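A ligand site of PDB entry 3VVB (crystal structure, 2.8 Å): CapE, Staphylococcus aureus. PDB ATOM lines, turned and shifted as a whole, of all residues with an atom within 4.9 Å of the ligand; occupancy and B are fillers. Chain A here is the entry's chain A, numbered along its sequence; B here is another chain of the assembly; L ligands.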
ATOM      1  N   THR A  31     -18.387 -25.175  25.125  1.00  0.00           N
ATOM      2  CA  THR A  31     -19.083 -26.368  24.614  1.00  0.00           C
ATOM      3  C   THR A  31     -18.350 -26.816  23.365  1.00  0.00           C
ATOM      4  O   THR A  31     -17.873 -25.995  22.602  1.00  0.00           O
ATOM      5  CB  THR A  31     -20.513 -26.098  24.185  1.00  0.00           C
ATOM      6  OG1 THR A  31     -20.475 -25.444  22.903  1.00  0.00           O
ATOM      7  CG2 THR A  31     -21.255 -25.245  25.217  1.00  0.00           C
ATOM      8  N   GLY A  32     -18.287 -28.123  23.143  1.00  0.00           N
ATOM      9  CA  GLY A  32     -17.382 -28.664  22.137  1.00  0.00           C
ATOM     10  C   GLY A  32     -15.948 -28.308  22.461  1.00  0.00           C
ATOM     11  O   GLY A  32     -15.118 -28.124  21.564  1.00  0.00           O
ATOM     12  N   THR A  34     -13.376 -29.762  23.242  1.00  0.00           N
ATOM     13  CA  THR A  34     -12.303 -30.701  22.889  1.00  0.00           C
ATOM     14  C   THR A  34     -11.830 -30.546  21.437  1.00  0.00           C
ATOM     15  O   THR A  34     -11.016 -31.343  20.972  1.00  0.00           O
ATOM     16  CB  THR A  34     -12.767 -32.159  23.103  1.00  0.00           C
ATOM     17  OG1 THR A  34     -14.057 -32.343  22.512  1.00  0.00           O
ATOM     18  CG2 THR A  34     -12.815 -32.487  24.600  1.00  0.00           C
ATOM     19  N   GLY A  35     -12.348 -29.548  20.731  1.00  0.00           N
ATOM     20  CA  GLY A  35     -12.081 -29.403  19.310  1.00  0.00           C
ATOM     21  C   GLY A  35     -10.824 -28.630  18.994  1.00  0.00           C
ATOM     22  O   GLY A  35     -10.115 -28.172  19.894  1.00  0.00           O
ATOM     23  N   SER A  36     -10.550 -28.503  17.694  1.00  0.00           N
ATOM     24  CA  SER A  36      -9.454 -27.682  17.203  1.00  0.00           C
ATOM     25  C   SER A  36      -9.487 -26.295  17.861  1.00  0.00           C
ATOM     26  O   SER A  36      -8.467 -25.833  18.369  1.00  0.00           O
ATOM     27  CB  SER A  36      -9.543 -27.556  15.678  1.00  0.00           C
ATOM     28  OG  SER A  36      -8.849 -28.615  15.026  1.00  0.00           O
ATOM     29  N   PHE A  37     -10.661 -25.673  17.858  1.00  0.00           N
ATOM     30  CA  PHE A  37     -10.856 -24.345  18.412  1.00  0.00           C
ATOM     31  C   PHE A  37     -10.817 -24.287  19.934  1.00  0.00           C
ATOM     32  O   PHE A  37     -10.101 -23.466  20.501  1.00  0.00           O
ATOM     33  CB  PHE A  37     -12.152 -23.723  17.902  1.00  0.00           C
ATOM     34  CG  PHE A  37     -12.540 -22.458  18.620  1.00  0.00           C
ATOM     35  CD1 PHE A  37     -11.872 -21.263  18.358  1.00  0.00           C
ATOM     36  CD2 PHE A  37     -13.574 -22.469  19.562  1.00  0.00           C
ATOM     37  CE1 PHE A  37     -12.231 -20.083  19.009  1.00  0.00           C
ATOM     38  CE2 PHE A  37     -13.941 -21.291  20.218  1.00  0.00           C
ATOM     39  CZ  PHE A  37     -13.253 -20.105  19.944  1.00  0.00           C
ATOM     40  N   GLY A  38     -11.592 -25.154  20.591  1.00  0.00           N
ATOM     41  CA  GLY A  38     -11.585 -25.249  22.055  1.00  0.00           C
ATOM     42  C   GLY A  38     -10.171 -25.271  22.602  1.00  0.00           C
ATOM     43  O   GLY A  38      -9.853 -24.569  23.570  1.00  0.00           O
ATOM     44  N   PHE A  56     -16.613 -28.669  28.006  1.00  0.00           N
ATOM     45  CA  PHE A  56     -17.853 -29.429  27.970  1.00  0.00           C
ATOM     46  C   PHE A  56     -17.965 -30.106  26.618  1.00  0.00           C
ATOM     47  O   PHE A  56     -17.971 -29.424  25.598  1.00  0.00           O
ATOM     48  CB  PHE A  56     -19.010 -28.456  28.158  1.00  0.00           C
ATOM     49  CG  PHE A  56     -20.371 -29.070  28.009  1.00  0.00           C
ATOM     50  CD1 PHE A  56     -21.027 -29.581  29.099  1.00  0.00           C
ATOM     51  CD2 PHE A  56     -21.019 -29.062  26.789  1.00  0.00           C
ATOM     52  CE1 PHE A  56     -22.309 -30.114  28.968  1.00  0.00           C
ATOM     53  CE2 PHE A  56     -22.298 -29.579  26.653  1.00  0.00           C
ATOM     54  CZ  PHE A  56     -22.938 -30.115  27.754  1.00  0.00           C
ATOM     55  N   SER A  57     -18.033 -31.439  26.622  1.00  0.00           N
ATOM     56  CA  SER A  57     -18.193 -32.209  25.389  1.00  0.00           C
ATOM     57  C   SER A  57     -18.580 -33.655  25.695  1.00  0.00           C
ATOM     58  O   SER A  57     -18.682 -34.050  26.849  1.00  0.00           O
ATOM     59  CB  SER A  57     -16.929 -32.156  24.532  1.00  0.00           C
ATOM     60  OG  SER A  57     -15.958 -33.093  24.989  1.00  0.00           O
ATOM     61  N   ARG A  58     -18.802 -34.428  24.636  1.00  0.00           N
ATOM     62  CA  ARG A  58     -19.258 -35.812  24.737  1.00  0.00           C
ATOM     63  C   ARG A  58     -18.129 -36.799  25.040  1.00  0.00           C
ATOM     64  O   ARG A  58     -18.360 -37.766  25.742  1.00  0.00           O
ATOM     65  CB  ARG A  58     -19.947 -36.263  23.438  1.00  0.00           C
ATOM     66  CG  ARG A  58     -21.029 -35.345  22.825  1.00  0.00           C
ATOM     67  CD  ARG A  58     -21.170 -35.589  21.311  1.00  0.00           C
ATOM     68  NE  ARG A  58     -19.947 -35.235  20.546  1.00  0.00           N
ATOM     69  CZ  ARG A  58     -19.748 -35.446  19.241  1.00  0.00           C
ATOM     70  NH1 ARG A  58     -20.672 -36.026  18.501  1.00  0.00           N
ATOM     71  NH2 ARG A  58     -18.591 -35.112  18.656  1.00  0.00           N
ATOM     72  N   ASP A  59     -16.935 -36.559  24.497  1.00  0.00           N
ATOM     73  CA  ASP A  59     -15.855 -37.558  24.401  1.00  0.00           C
ATOM     74  C   ASP A  59     -14.866 -37.568  25.557  1.00  0.00           C
ATOM     75  O   ASP A  59     -13.963 -36.731  25.642  1.00  0.00           O
ATOM     76  CB  ASP A  59     -15.103 -37.437  23.064  1.00  0.00           C
ATOM     77  CG  ASP A  59     -13.975 -38.500  22.885  1.00  0.00           C
ATOM     78  OD1 ASP A  59     -12.996 -38.198  22.169  1.00  0.00           O
ATOM     79  OD2 ASP A  59     -14.070 -39.642  23.434  1.00  0.00           O
ATOM     80  N   LYS A  62     -10.908 -37.656  24.389  1.00  0.00           N
ATOM     81  CA  LYS A  62     -10.257 -36.384  24.102  1.00  0.00           C
ATOM     82  C   LYS A  62     -10.073 -35.610  25.404  1.00  0.00           C
ATOM     83  O   LYS A  62      -8.973 -35.130  25.698  1.00  0.00           O
ATOM     84  CB  LYS A  62     -11.024 -35.591  23.046  1.00  0.00           C
ATOM     85  CG  LYS A  62     -10.639 -35.949  21.599  1.00  0.00           C
ATOM     86  CD  LYS A  62     -11.466 -35.168  20.578  1.00  0.00           C
ATOM     87  CE  LYS A  62     -12.698 -35.938  20.120  1.00  0.00           C
ATOM     88  NZ  LYS A  62     -13.833 -35.034  19.826  1.00  0.00           N
ATOM     89  N   GLY A  80     -21.023 -34.166  28.895  1.00  0.00           N
ATOM     90  CA  GLY A  80     -22.391 -33.802  28.591  1.00  0.00           C
ATOM     91  C   GLY A  80     -22.507 -33.583  27.122  1.00  0.00           C
ATOM     92  O   GLY A  80     -21.494 -33.567  26.429  1.00  0.00           O
ATOM     93  N   ASP A  81     -23.728 -33.433  26.611  1.00  0.00           N
ATOM     94  CA  ASP A  81     -23.879 -32.977  25.232  1.00  0.00           C
ATOM     95  C   ASP A  81     -25.048 -32.013  25.004  1.00  0.00           C
ATOM     96  O   ASP A  81     -26.018 -32.011  25.760  1.00  0.00           O
ATOM     97  CB  ASP A  81     -23.839 -34.148  24.229  1.00  0.00           C
ATOM     98  CG  ASP A  81     -25.134 -34.374  23.560  1.00  0.00           C
ATOM     99  OD1 ASP A  81     -25.336 -33.914  22.425  1.00  0.00           O
ATOM    100  OD2 ASP A  81     -25.970 -35.006  24.170  1.00  0.00           O
ATOM    101  N   VAL A  82     -24.928 -31.168  23.981  1.00  0.00           N
ATOM    102  CA  VAL A  82     -25.740 -29.941  23.878  1.00  0.00           C
ATOM    103  C   VAL A  82     -27.172 -30.286  23.491  1.00  0.00           C
ATOM    104  O   VAL A  82     -28.092 -29.469  23.600  1.00  0.00           O
ATOM    105  CB  VAL A  82     -25.099 -28.852  22.966  1.00  0.00           C
ATOM    106  CG1 VAL A  82     -23.728 -28.480  23.505  1.00  0.00           C
ATOM    107  CG2 VAL A  82     -25.011 -29.297  21.515  1.00  0.00           C
ATOM    108  N   ARG A  83     -27.324 -31.520  23.015  1.00  0.00           N
ATOM    109  CA  ARG A  83     -28.611 -32.085  22.727  1.00  0.00           C
ATOM    110  C   ARG A  83     -29.440 -32.218  23.973  1.00  0.00           C
ATOM    111  O   ARG A  83     -30.660 -32.195  23.873  1.00  0.00           O
ATOM    112  CB  ARG A  83     -28.434 -33.412  22.011  1.00  0.00           C
ATOM    113  CG  ARG A  83     -28.607 -33.245  20.529  1.00  0.00           C
ATOM    114  CD  ARG A  83     -27.497 -33.798  19.669  1.00  0.00           C
ATOM    115  NE  ARG A  83     -27.846 -35.097  19.159  1.00  0.00           N
ATOM    116  CZ  ARG A  83     -27.569 -35.532  17.931  1.00  0.00           C
ATOM    117  NH1 ARG A  83     -26.936 -34.749  17.048  1.00  0.00           N
ATOM    118  NH2 ARG A  83     -27.924 -36.749  17.569  1.00  0.00           N
ATOM    119  N   ALA A 101     -19.028 -23.721  20.775  1.00  0.00           N
ATOM    120  CA  ALA A 101     -18.280 -24.265  19.627  1.00  0.00           C
ATOM    121  C   ALA A 101     -18.733 -25.700  19.212  1.00  0.00           C
ATOM    122  O   ALA A 101     -18.145 -26.302  18.325  1.00  0.00           O
ATOM    123  CB  ALA A 101     -16.800 -24.256  19.932  1.00  0.00           C
ATOM    124  N   ALA A 102     -19.775 -26.224  19.852  1.00  0.00           N
ATOM    125  CA  ALA A 102     -20.184 -27.619  19.652  1.00  0.00           C
ATOM    126  C   ALA A 102     -20.985 -27.757  18.372  1.00  0.00           C
ATOM    127  O   ALA A 102     -22.040 -27.167  18.220  1.00  0.00           O
ATOM    128  CB  ALA A 102     -20.991 -28.105  20.843  1.00  0.00           C
ATOM    129  N   ALA A 103     -20.492 -28.531  17.422  1.00  0.00           N
ATOM    130  CA  ALA A 103     -21.204 -28.696  16.197  1.00  0.00           C
ATOM    131  C   ALA A 103     -20.822 -29.954  15.457  1.00  0.00           C
ATOM    132  O   ALA A 103     -19.768 -30.554  15.688  1.00  0.00           O
ATOM    133  CB  ALA A 103     -20.989 -27.503  15.278  1.00  0.00           C
ATOM    134  N   LYS A 105     -19.848 -30.372  11.998  1.00  0.00           N
ATOM    135  CA  LYS A 105     -19.274 -29.377  11.095  1.00  0.00           C
ATOM    136  C   LYS A 105     -18.707 -29.930   9.771  1.00  0.00           C
ATOM    137  O   LYS A 105     -18.222 -29.163   8.941  1.00  0.00           O
ATOM    138  CB  LYS A 105     -18.233 -28.527  11.831  1.00  0.00           C
ATOM    139  CG  LYS A 105     -17.033 -29.303  12.337  1.00  0.00           C
ATOM    140  CD  LYS A 105     -15.774 -28.448  12.197  1.00  0.00           C
ATOM    141  CE  LYS A 105     -14.521 -29.298  12.034  1.00  0.00           C
ATOM    142  NZ  LYS A 105     -13.290 -28.450  12.027  1.00  0.00           N
ATOM    143  N   THR A 120     -27.994 -30.948  16.784  1.00  0.00           N
ATOM    144  CA  THR A 120     -26.808 -30.421  17.436  1.00  0.00           C
ATOM    145  C   THR A 120     -26.677 -28.947  17.147  1.00  0.00           C
ATOM    146  O   THR A 120     -26.626 -28.145  18.077  1.00  0.00           O
ATOM    147  CB  THR A 120     -25.535 -31.116  16.886  1.00  0.00           C
ATOM    148  OG1 THR A 120     -25.563 -32.523  17.187  1.00  0.00           O
ATOM    149  CG2 THR A 120     -24.291 -30.488  17.489  1.00  0.00           C
ATOM    150  N   LEU A 143     -20.113 -19.901  17.577  1.00  0.00           N
ATOM    151  CA  LEU A 143     -19.174 -19.992  16.465  1.00  0.00           C
ATOM    152  C   LEU A 143     -19.906 -20.441  15.196  1.00  0.00           C
ATOM    153  O   LEU A 143     -20.648 -21.404  15.202  1.00  0.00           O
ATOM    154  CB  LEU A 143     -17.999 -20.945  16.809  1.00  0.00           C
ATOM    155  CG  LEU A 143     -16.888 -20.678  17.852  1.00  0.00           C
ATOM    156  CD1 LEU A 143     -15.714 -19.996  17.181  1.00  0.00           C
ATOM    157  CD2 LEU A 143     -17.255 -19.924  19.134  1.00  0.00           C
ATOM    158  N   SER A 144     -19.723 -19.694  14.111  1.00  0.00           N
ATOM    159  CA  SER A 144     -20.369 -20.000  12.845  1.00  0.00           C
ATOM    160  C   SER A 144     -19.354 -20.045  11.700  1.00  0.00           C
ATOM    161  O   SER A 144     -18.146 -20.010  11.929  1.00  0.00           O
ATOM    162  CB  SER A 144     -21.469 -18.983  12.560  1.00  0.00           C
ATOM    163  OG  SER A 144     -22.269 -19.409  11.483  1.00  0.00           O
ATOM    164  N   THR A 145     -19.851 -20.132  10.468  1.00  0.00           N
ATOM    165  CA  THR A 145     -19.010 -20.413   9.317  1.00  0.00           C
ATOM    166  C   THR A 145     -19.464 -19.689   8.063  1.00  0.00           C
ATOM    167  O   THR A 145     -20.663 -19.537   7.823  1.00  0.00           O
ATOM    168  CB  THR A 145     -18.998 -21.923   9.024  1.00  0.00           C
ATOM    169  OG1 THR A 145     -18.307 -22.156   7.796  1.00  0.00           O
ATOM    170  CG2 THR A 145     -20.418 -22.452   8.884  1.00  0.00           C
ATOM    171  N   ASP A 146     -18.492 -19.290   7.258  1.00  0.00           N
ATOM    172  CA  ASP A 146     -18.762 -18.702   5.949  1.00  0.00           C
ATOM    173  C   ASP A 146     -19.755 -19.497   5.110  1.00  0.00           C
ATOM    174  O   ASP A 146     -20.404 -18.957   4.223  1.00  0.00           O
ATOM    175  CB  ASP A 146     -17.462 -18.539   5.170  1.00  0.00           C
ATOM    176  CG  ASP A 146     -16.764 -19.865   4.908  1.00  0.00           C
ATOM    177  OD1 ASP A 146     -16.831 -20.776   5.765  1.00  0.00           O
ATOM    178  OD2 ASP A 146     -16.112 -19.976   3.852  1.00  0.00           O
ATOM    179  N   LYS A 159     -26.203 -24.244   9.939  1.00  0.00           N
ATOM    180  CA  LYS A 159     -25.477 -23.112  10.517  1.00  0.00           C
ATOM    181  C   LYS A 159     -26.166 -21.786  10.312  1.00  0.00           C
ATOM    182  O   LYS A 159     -26.283 -20.989  11.239  1.00  0.00           O
ATOM    183  CB  LYS A 159     -24.063 -23.042   9.953  1.00  0.00           C
ATOM    184  CG  LYS A 159     -23.151 -24.062  10.587  1.00  0.00           C
ATOM    185  CD  LYS A 159     -23.121 -23.828  12.086  1.00  0.00           C
ATOM    186  CE  LYS A 159     -21.961 -24.567  12.675  1.00  0.00           C
ATOM    187  NZ  LYS A 159     -21.627 -24.024  14.024  1.00  0.00           N
ATOM    188  N   TYR A 185     -16.419 -17.747  10.475  1.00  0.00           N
ATOM    189  CA  TYR A 185     -15.166 -17.785   9.770  1.00  0.00           C
ATOM    190  C   TYR A 185     -15.046 -18.826   8.690  1.00  0.00           C
ATOM    191  O   TYR A 185     -15.741 -19.834   8.705  1.00  0.00           O
ATOM    192  CB  TYR A 185     -13.958 -17.793  10.686  1.00  0.00           C
ATOM    193  CG  TYR A 185     -13.905 -18.776  11.810  1.00  0.00           C
ATOM    194  CD1 TYR A 185     -13.446 -20.071  11.604  1.00  0.00           C
ATOM    195  CD2 TYR A 185     -14.187 -18.368  13.124  1.00  0.00           C
ATOM    196  CE1 TYR A 185     -13.330 -20.966  12.662  1.00  0.00           C
ATOM    197  CE2 TYR A 185     -14.075 -19.250  14.182  1.00  0.00           C
ATOM    198  CZ  TYR A 185     -13.647 -20.552  13.948  1.00  0.00           C
ATOM    199  OH  TYR A 185     -13.528 -21.432  15.000  1.00  0.00           O
ATOM    200  N   GLY A 186     -14.167 -18.521   7.739  1.00  0.00           N
ATOM    201  CA  GLY A 186     -13.827 -19.439   6.676  1.00  0.00           C
ATOM    202  C   GLY A 186     -12.918 -20.494   7.258  1.00  0.00           C
ATOM    203  O   GLY A 186     -12.871 -20.672   8.481  1.00  0.00           O
ATOM    204  N   ASN A 187     -12.171 -21.161   6.383  1.00  0.00           N
ATOM    205  CA  ASN A 187     -11.313 -22.261   6.790  1.00  0.00           C
ATOM    206  C   ASN A 187     -10.075 -21.796   7.537  1.00  0.00           C
ATOM    207  O   ASN A 187      -9.522 -20.744   7.232  1.00  0.00           O
ATOM    208  CB  ASN A 187     -10.906 -23.094   5.580  1.00  0.00           C
ATOM    209  CG  ASN A 187     -10.513 -24.513   5.954  1.00  0.00           C
ATOM    210  OD1 ASN A 187      -9.340 -24.869   5.933  1.00  0.00           O
ATOM    211  ND2 ASN A 187     -11.503 -25.335   6.310  1.00  0.00           N
ATOM    212  N   VAL A 188      -9.670 -22.575   8.530  1.00  0.00           N
ATOM    213  CA  VAL A 188      -8.447 -22.321   9.288  1.00  0.00           C
ATOM    214  C   VAL A 188      -7.411 -23.390   8.965  1.00  0.00           C
ATOM    215  O   VAL A 188      -7.785 -24.501   8.572  1.00  0.00           O
ATOM    216  CB  VAL A 188      -8.702 -22.246  10.820  1.00  0.00           C
ATOM    217  CG1 VAL A 188      -9.991 -21.501  11.129  1.00  0.00           C
ATOM    218  CG2 VAL A 188      -8.714 -23.625  11.446  1.00  0.00           C
ATOM    219  N   ASP B  59     -19.026 -39.267  16.557  1.00  0.00           N
ATOM    220  CA  ASP B  59     -17.890 -38.437  16.123  1.00  0.00           C
ATOM    221  C   ASP B  59     -17.536 -38.529  14.646  1.00  0.00           C
ATOM    222  O   ASP B  59     -16.889 -39.479  14.202  1.00  0.00           O
ATOM    223  CB  ASP B  59     -16.638 -38.711  16.999  1.00  0.00           C
ATOM    224  CG  ASP B  59     -15.421 -37.821  16.613  1.00  0.00           C
ATOM    225  OD1 ASP B  59     -14.272 -38.297  16.819  1.00  0.00           O
ATOM    226  OD2 ASP B  59     -15.576 -36.666  16.115  1.00  0.00           O
ATOM    227  N   GLU B  60     -17.922 -37.491  13.911  1.00  0.00           N
ATOM    228  CA  GLU B  60     -17.603 -37.345  12.490  1.00  0.00           C
ATOM    229  C   GLU B  60     -16.092 -37.354  12.192  1.00  0.00           C
ATOM    230  O   GLU B  60     -15.679 -37.755  11.090  1.00  0.00           O
ATOM    231  CB  GLU B  60     -18.228 -36.053  11.941  1.00  0.00           C
ATOM    232  CG  GLU B  60     -17.958 -34.823  12.814  1.00  0.00           C
ATOM    233  CD  GLU B  60     -18.383 -33.505  12.182  1.00  0.00           C
ATOM    234  OE1 GLU B  60     -18.123 -32.437  12.800  1.00  0.00           O
ATOM    235  OE2 GLU B  60     -18.970 -33.528  11.081  1.00  0.00           O
ATOM    236  N   LYS B  61     -15.279 -36.898  13.143  1.00  0.00           N
ATOM    237  CA  LYS B  61     -13.814 -36.836  12.953  1.00  0.00           C
ATOM    238  C   LYS B  61     -13.192 -38.230  12.920  1.00  0.00           C
ATOM    239  O   LYS B  61     -12.435 -38.553  11.999  1.00  0.00           O
ATOM    240  CB  LYS B  61     -13.131 -35.965  14.013  1.00  0.00           C
ATOM    241  CG  LYS B  61     -13.254 -34.465  13.793  1.00  0.00           C
ATOM    242  CD  LYS B  61     -12.526 -33.647  14.857  1.00  0.00           C
ATOM    243  CE  LYS B  61     -13.207 -33.690  16.219  1.00  0.00           C
ATOM    244  NZ  LYS B  61     -12.307 -33.153  17.287  1.00  0.00           N
HETATM  245  P1  LIG L   1     -13.934 -29.305  15.976  1.00  0.00           P
HETATM  246  O1  LIG L   1     -12.439 -29.290  16.217  1.00  0.00           O
HETATM  247  O2  LIG L   1     -14.585 -30.477  15.257  1.00  0.00           O
HETATM  248  O3  LIG L   1     -14.639 -29.033  17.391  1.00  0.00           O
HETATM  249  C1  LIG L   1     -16.027 -29.286  17.584  1.00  0.00           C
HETATM  250  C2  LIG L   1     -16.170 -29.930  18.938  1.00  0.00           C
HETATM  251  O4  LIG L   1     -17.549 -30.008  19.236  1.00  0.00           O
HETATM  252  C3  LIG L   1     -15.632 -31.355  19.038  1.00  0.00           C
HETATM  253  O5  LIG L   1     -14.428 -31.366  19.827  1.00  0.00           O
HETATM  254  C4  LIG L   1     -16.733 -32.156  19.721  1.00  0.00           C
HETATM  255  O6  LIG L   1     -16.263 -32.688  20.942  1.00  0.00           O
HETATM  256  C5  LIG L   1     -17.751 -31.114  20.106  1.00  0.00           C
HETATM  257  N1  LIG L   1     -19.146 -31.570  19.997  1.00  0.00           N
HETATM  258  C6  LIG L   1     -19.760 -32.036  18.893  1.00  0.00           C
HETATM  259  N2  LIG L   1     -21.057 -32.339  19.169  1.00  0.00           N
HETATM  260  C7  LIG L   1     -21.288 -32.018  20.462  1.00  0.00           C
HETATM  261  C8  LIG L   1     -22.431 -32.090  21.386  1.00  0.00           C
HETATM  262  N3  LIG L   1     -23.611 -32.557  20.938  1.00  0.00           N
HETATM  263  N4  LIG L   1     -22.262 -31.681  22.663  1.00  0.00           N
HETATM  264  C9  LIG L   1     -21.073 -31.202  23.094  1.00  0.00           C
HETATM  265  N5  LIG L   1     -19.966 -31.118  22.316  1.00  0.00           N
HETATM  266  C10 LIG L   1     -20.016 -31.513  21.014  1.00  0.00           C
HETATM  267  O7  LIG L   1     -14.275 -27.955  15.159  1.00  0.00           O
HETATM  268  P2  LIG L   1     -13.602 -26.543  15.564  1.00  0.00           P
HETATM  269  O8  LIG L   1     -12.458 -26.257  14.613  1.00  0.00           O
HETATM  270  O9  LIG L   1     -13.355 -26.556  17.073  1.00  0.00           O
HETATM  271  O10 LIG L   1     -14.782 -25.518  15.211  1.00  0.00           O
HETATM  272  C11 LIG L   1     -15.807 -25.164  16.149  1.00  0.00           C
HETATM  273  C12 LIG L   1     -16.808 -24.235  15.478  1.00  0.00           C
HETATM  274  O11 LIG L   1     -16.166 -23.294  14.589  1.00  0.00           O
HETATM  275  C13 LIG L   1     -17.776 -25.083  14.666  1.00  0.00           C
HETATM  276  O12 LIG L   1     -19.130 -24.826  15.091  1.00  0.00           O
HETATM  277  C14 LIG L   1     -17.569 -24.644  13.222  1.00  0.00           C
HETATM  278  O13 LIG L   1     -18.808 -24.513  12.508  1.00  0.00           O
HETATM  279  C15 LIG L   1     -16.790 -23.327  13.280  1.00  0.00           C
HETATM  280  N6  LIG L   1     -15.896 -23.266  12.106  1.00  0.00           N
HETATM  281  C16 LIG L   1     -14.750 -23.998  12.060  1.00  0.00           C
HETATM  282  C17 LIG L   1     -13.917 -23.957  10.932  1.00  0.00           C
HETATM  283  C18 LIG L   1     -12.655 -24.780  10.898  1.00  0.00           C
HETATM  284  O14 LIG L   1     -12.071 -25.065  11.929  1.00  0.00           O
HETATM  285  N7  LIG L   1     -12.196 -25.194   9.713  1.00  0.00           N
HETATM  286  C19 LIG L   1     -14.275 -23.154   9.841  1.00  0.00           C
HETATM  287  C20 LIG L   1     -15.448 -22.416   9.905  1.00  0.00           C
HETATM  288  C21 LIG L   1     -16.239 -22.497  11.054  1.00  0.00           C
HETATM  289  P3  LIG L   1     -16.743 -34.128  21.486  1.00  0.00           P
HETATM  290  O15 LIG L   1     -16.583 -35.048  20.271  1.00  0.00           O
HETATM  291  O16 LIG L   1     -15.735 -34.380  22.598  1.00  0.00           O
HETATM  292  O17 LIG L   1     -18.152 -33.899  21.998  1.00  0.00           O
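An oxygen (O1) of the ligand sits at hydrogen-bond distance from the backbone NH (N) of Ser 36, at 2.5 Å.
The backbone NH (N) of Arg 58 sits at hydrogen-bond distance from an oxygen (O17) of the ligand, at 2.8 Å.
O15 of the ligand is in salt-bridge range of NH2 of Arg 58.
O16 of the ligand sits at hydrogen-bond distance from OG1 of Thr 34 (2.6 Å).
A nitrogen (N3) of the ligand is in hydrogen-bond range of the side-chain carboxylate (OD1) of Asp 81 (2.7 Å).
OG of Ser 57 sits at hydrogen-bond distance from O16 of the ligand (2.7 Å).
An oxygen (O15) of the ligand lies within salt-bridge range of the side-chain amino group (NZ) of Lys 62, at 2.8 Å.
NZ of Lys 159 lies within hydrogen-bond range of O12 of the ligand (2.8 Å).
The side-chain hydroxyl (OH) of Tyr 185 is in hydrogen-bond range of an oxygen (O11) of the ligand.
An oxygen (O5) of the ligand lies within hydrogen-bond range of the backbone NH (N) of Gly 35, at 2.9 Å.
The backbone NH (N) of Phe 37 is in hydrogen-bond range of an oxygen (O9) of the ligand (2.9 Å).
A nitrogen (N4) of the ligand sits at hydrogen-bond distance from the backbone NH (N) of Val 82, at 3.0 Å.
O16 of the ligand sits at hydrogen-bond distance from N of Asp 59 of chain A, 3.1 Å away.
The side-chain amino group (NZ) of Lys 105 is in salt-bridge range of an oxygen (O8) of the ligand, 3.5 Å away.
ND2 of Asn 187 lies close to N7 of the ligand (3.5 Å).
The backbone carbonyl oxygen of Gly 80 is in hydrogen-bond range of the backbone NH of Arg 58 (3.3 Å).
OG of Ser 57 is in hydrogen-bond range of OG1 of Thr 34 (3.2 Å).
The side-chain carboxylate of Asp 81 lies close to the backbone NH of Arg 83, 3.2 Å away.
The side-chain amino group (NZ) of Lys 159 is in hydrogen-bond range of the backbone carbonyl oxygen (O) of Leu 143.
N of Tyr 185 lies within hydrogen-bond range of O of Ser 144 (3.2 Å).
The backbone carbonyl oxygen (O) of Tyr 185 is in hydrogen-bond range of the backbone NH (N) of Asp 146 (3.2 Å).
OD1 of Asp 146 is in hydrogen-bond range of OG1 of Thr 145 (2.9 Å).
N of Ala 102 sits at hydrogen-bond distance from OG1 of Thr 31, 3.2 Å away.
Residues that only touch the ligand: Gly 186 (3.2 Å), Gly 32 (3.2 Å), Ser 144 (3.3 Å), Ala 103 (3.3 Å), Ala 101 (3.4 Å), Thr 145 (3.5 Å), Ala 102 (3.5 Å), Lys 61 of chain B (3.6 Å), Val 188 (3.7 Å) and Leu 143 (3.7 Å).
Hydrophobic or aromatic side chains that line the ligand: Phe 37, Val 82, Ala 102, Ala 103, Leu 143, Tyr 185 and Val 188.
Within 4 Å of the ligand: Gly 32, Thr 34, Gly 35, Ser 36, Phe 37, Ser 57, Arg 58, Asp 59 of chain A, Lys 62, Asp 81, Val 82, Ala 101, Ala 102, Ala 103, Lys 105, Leu 143, Ser 144, Thr 145, Lys 159, Tyr 185, Gly 186, Asn 187, Val 188 and Lys 61 of chain B.
Along chain A the residues within 4 Å of the ligand span positions 32 to 188.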
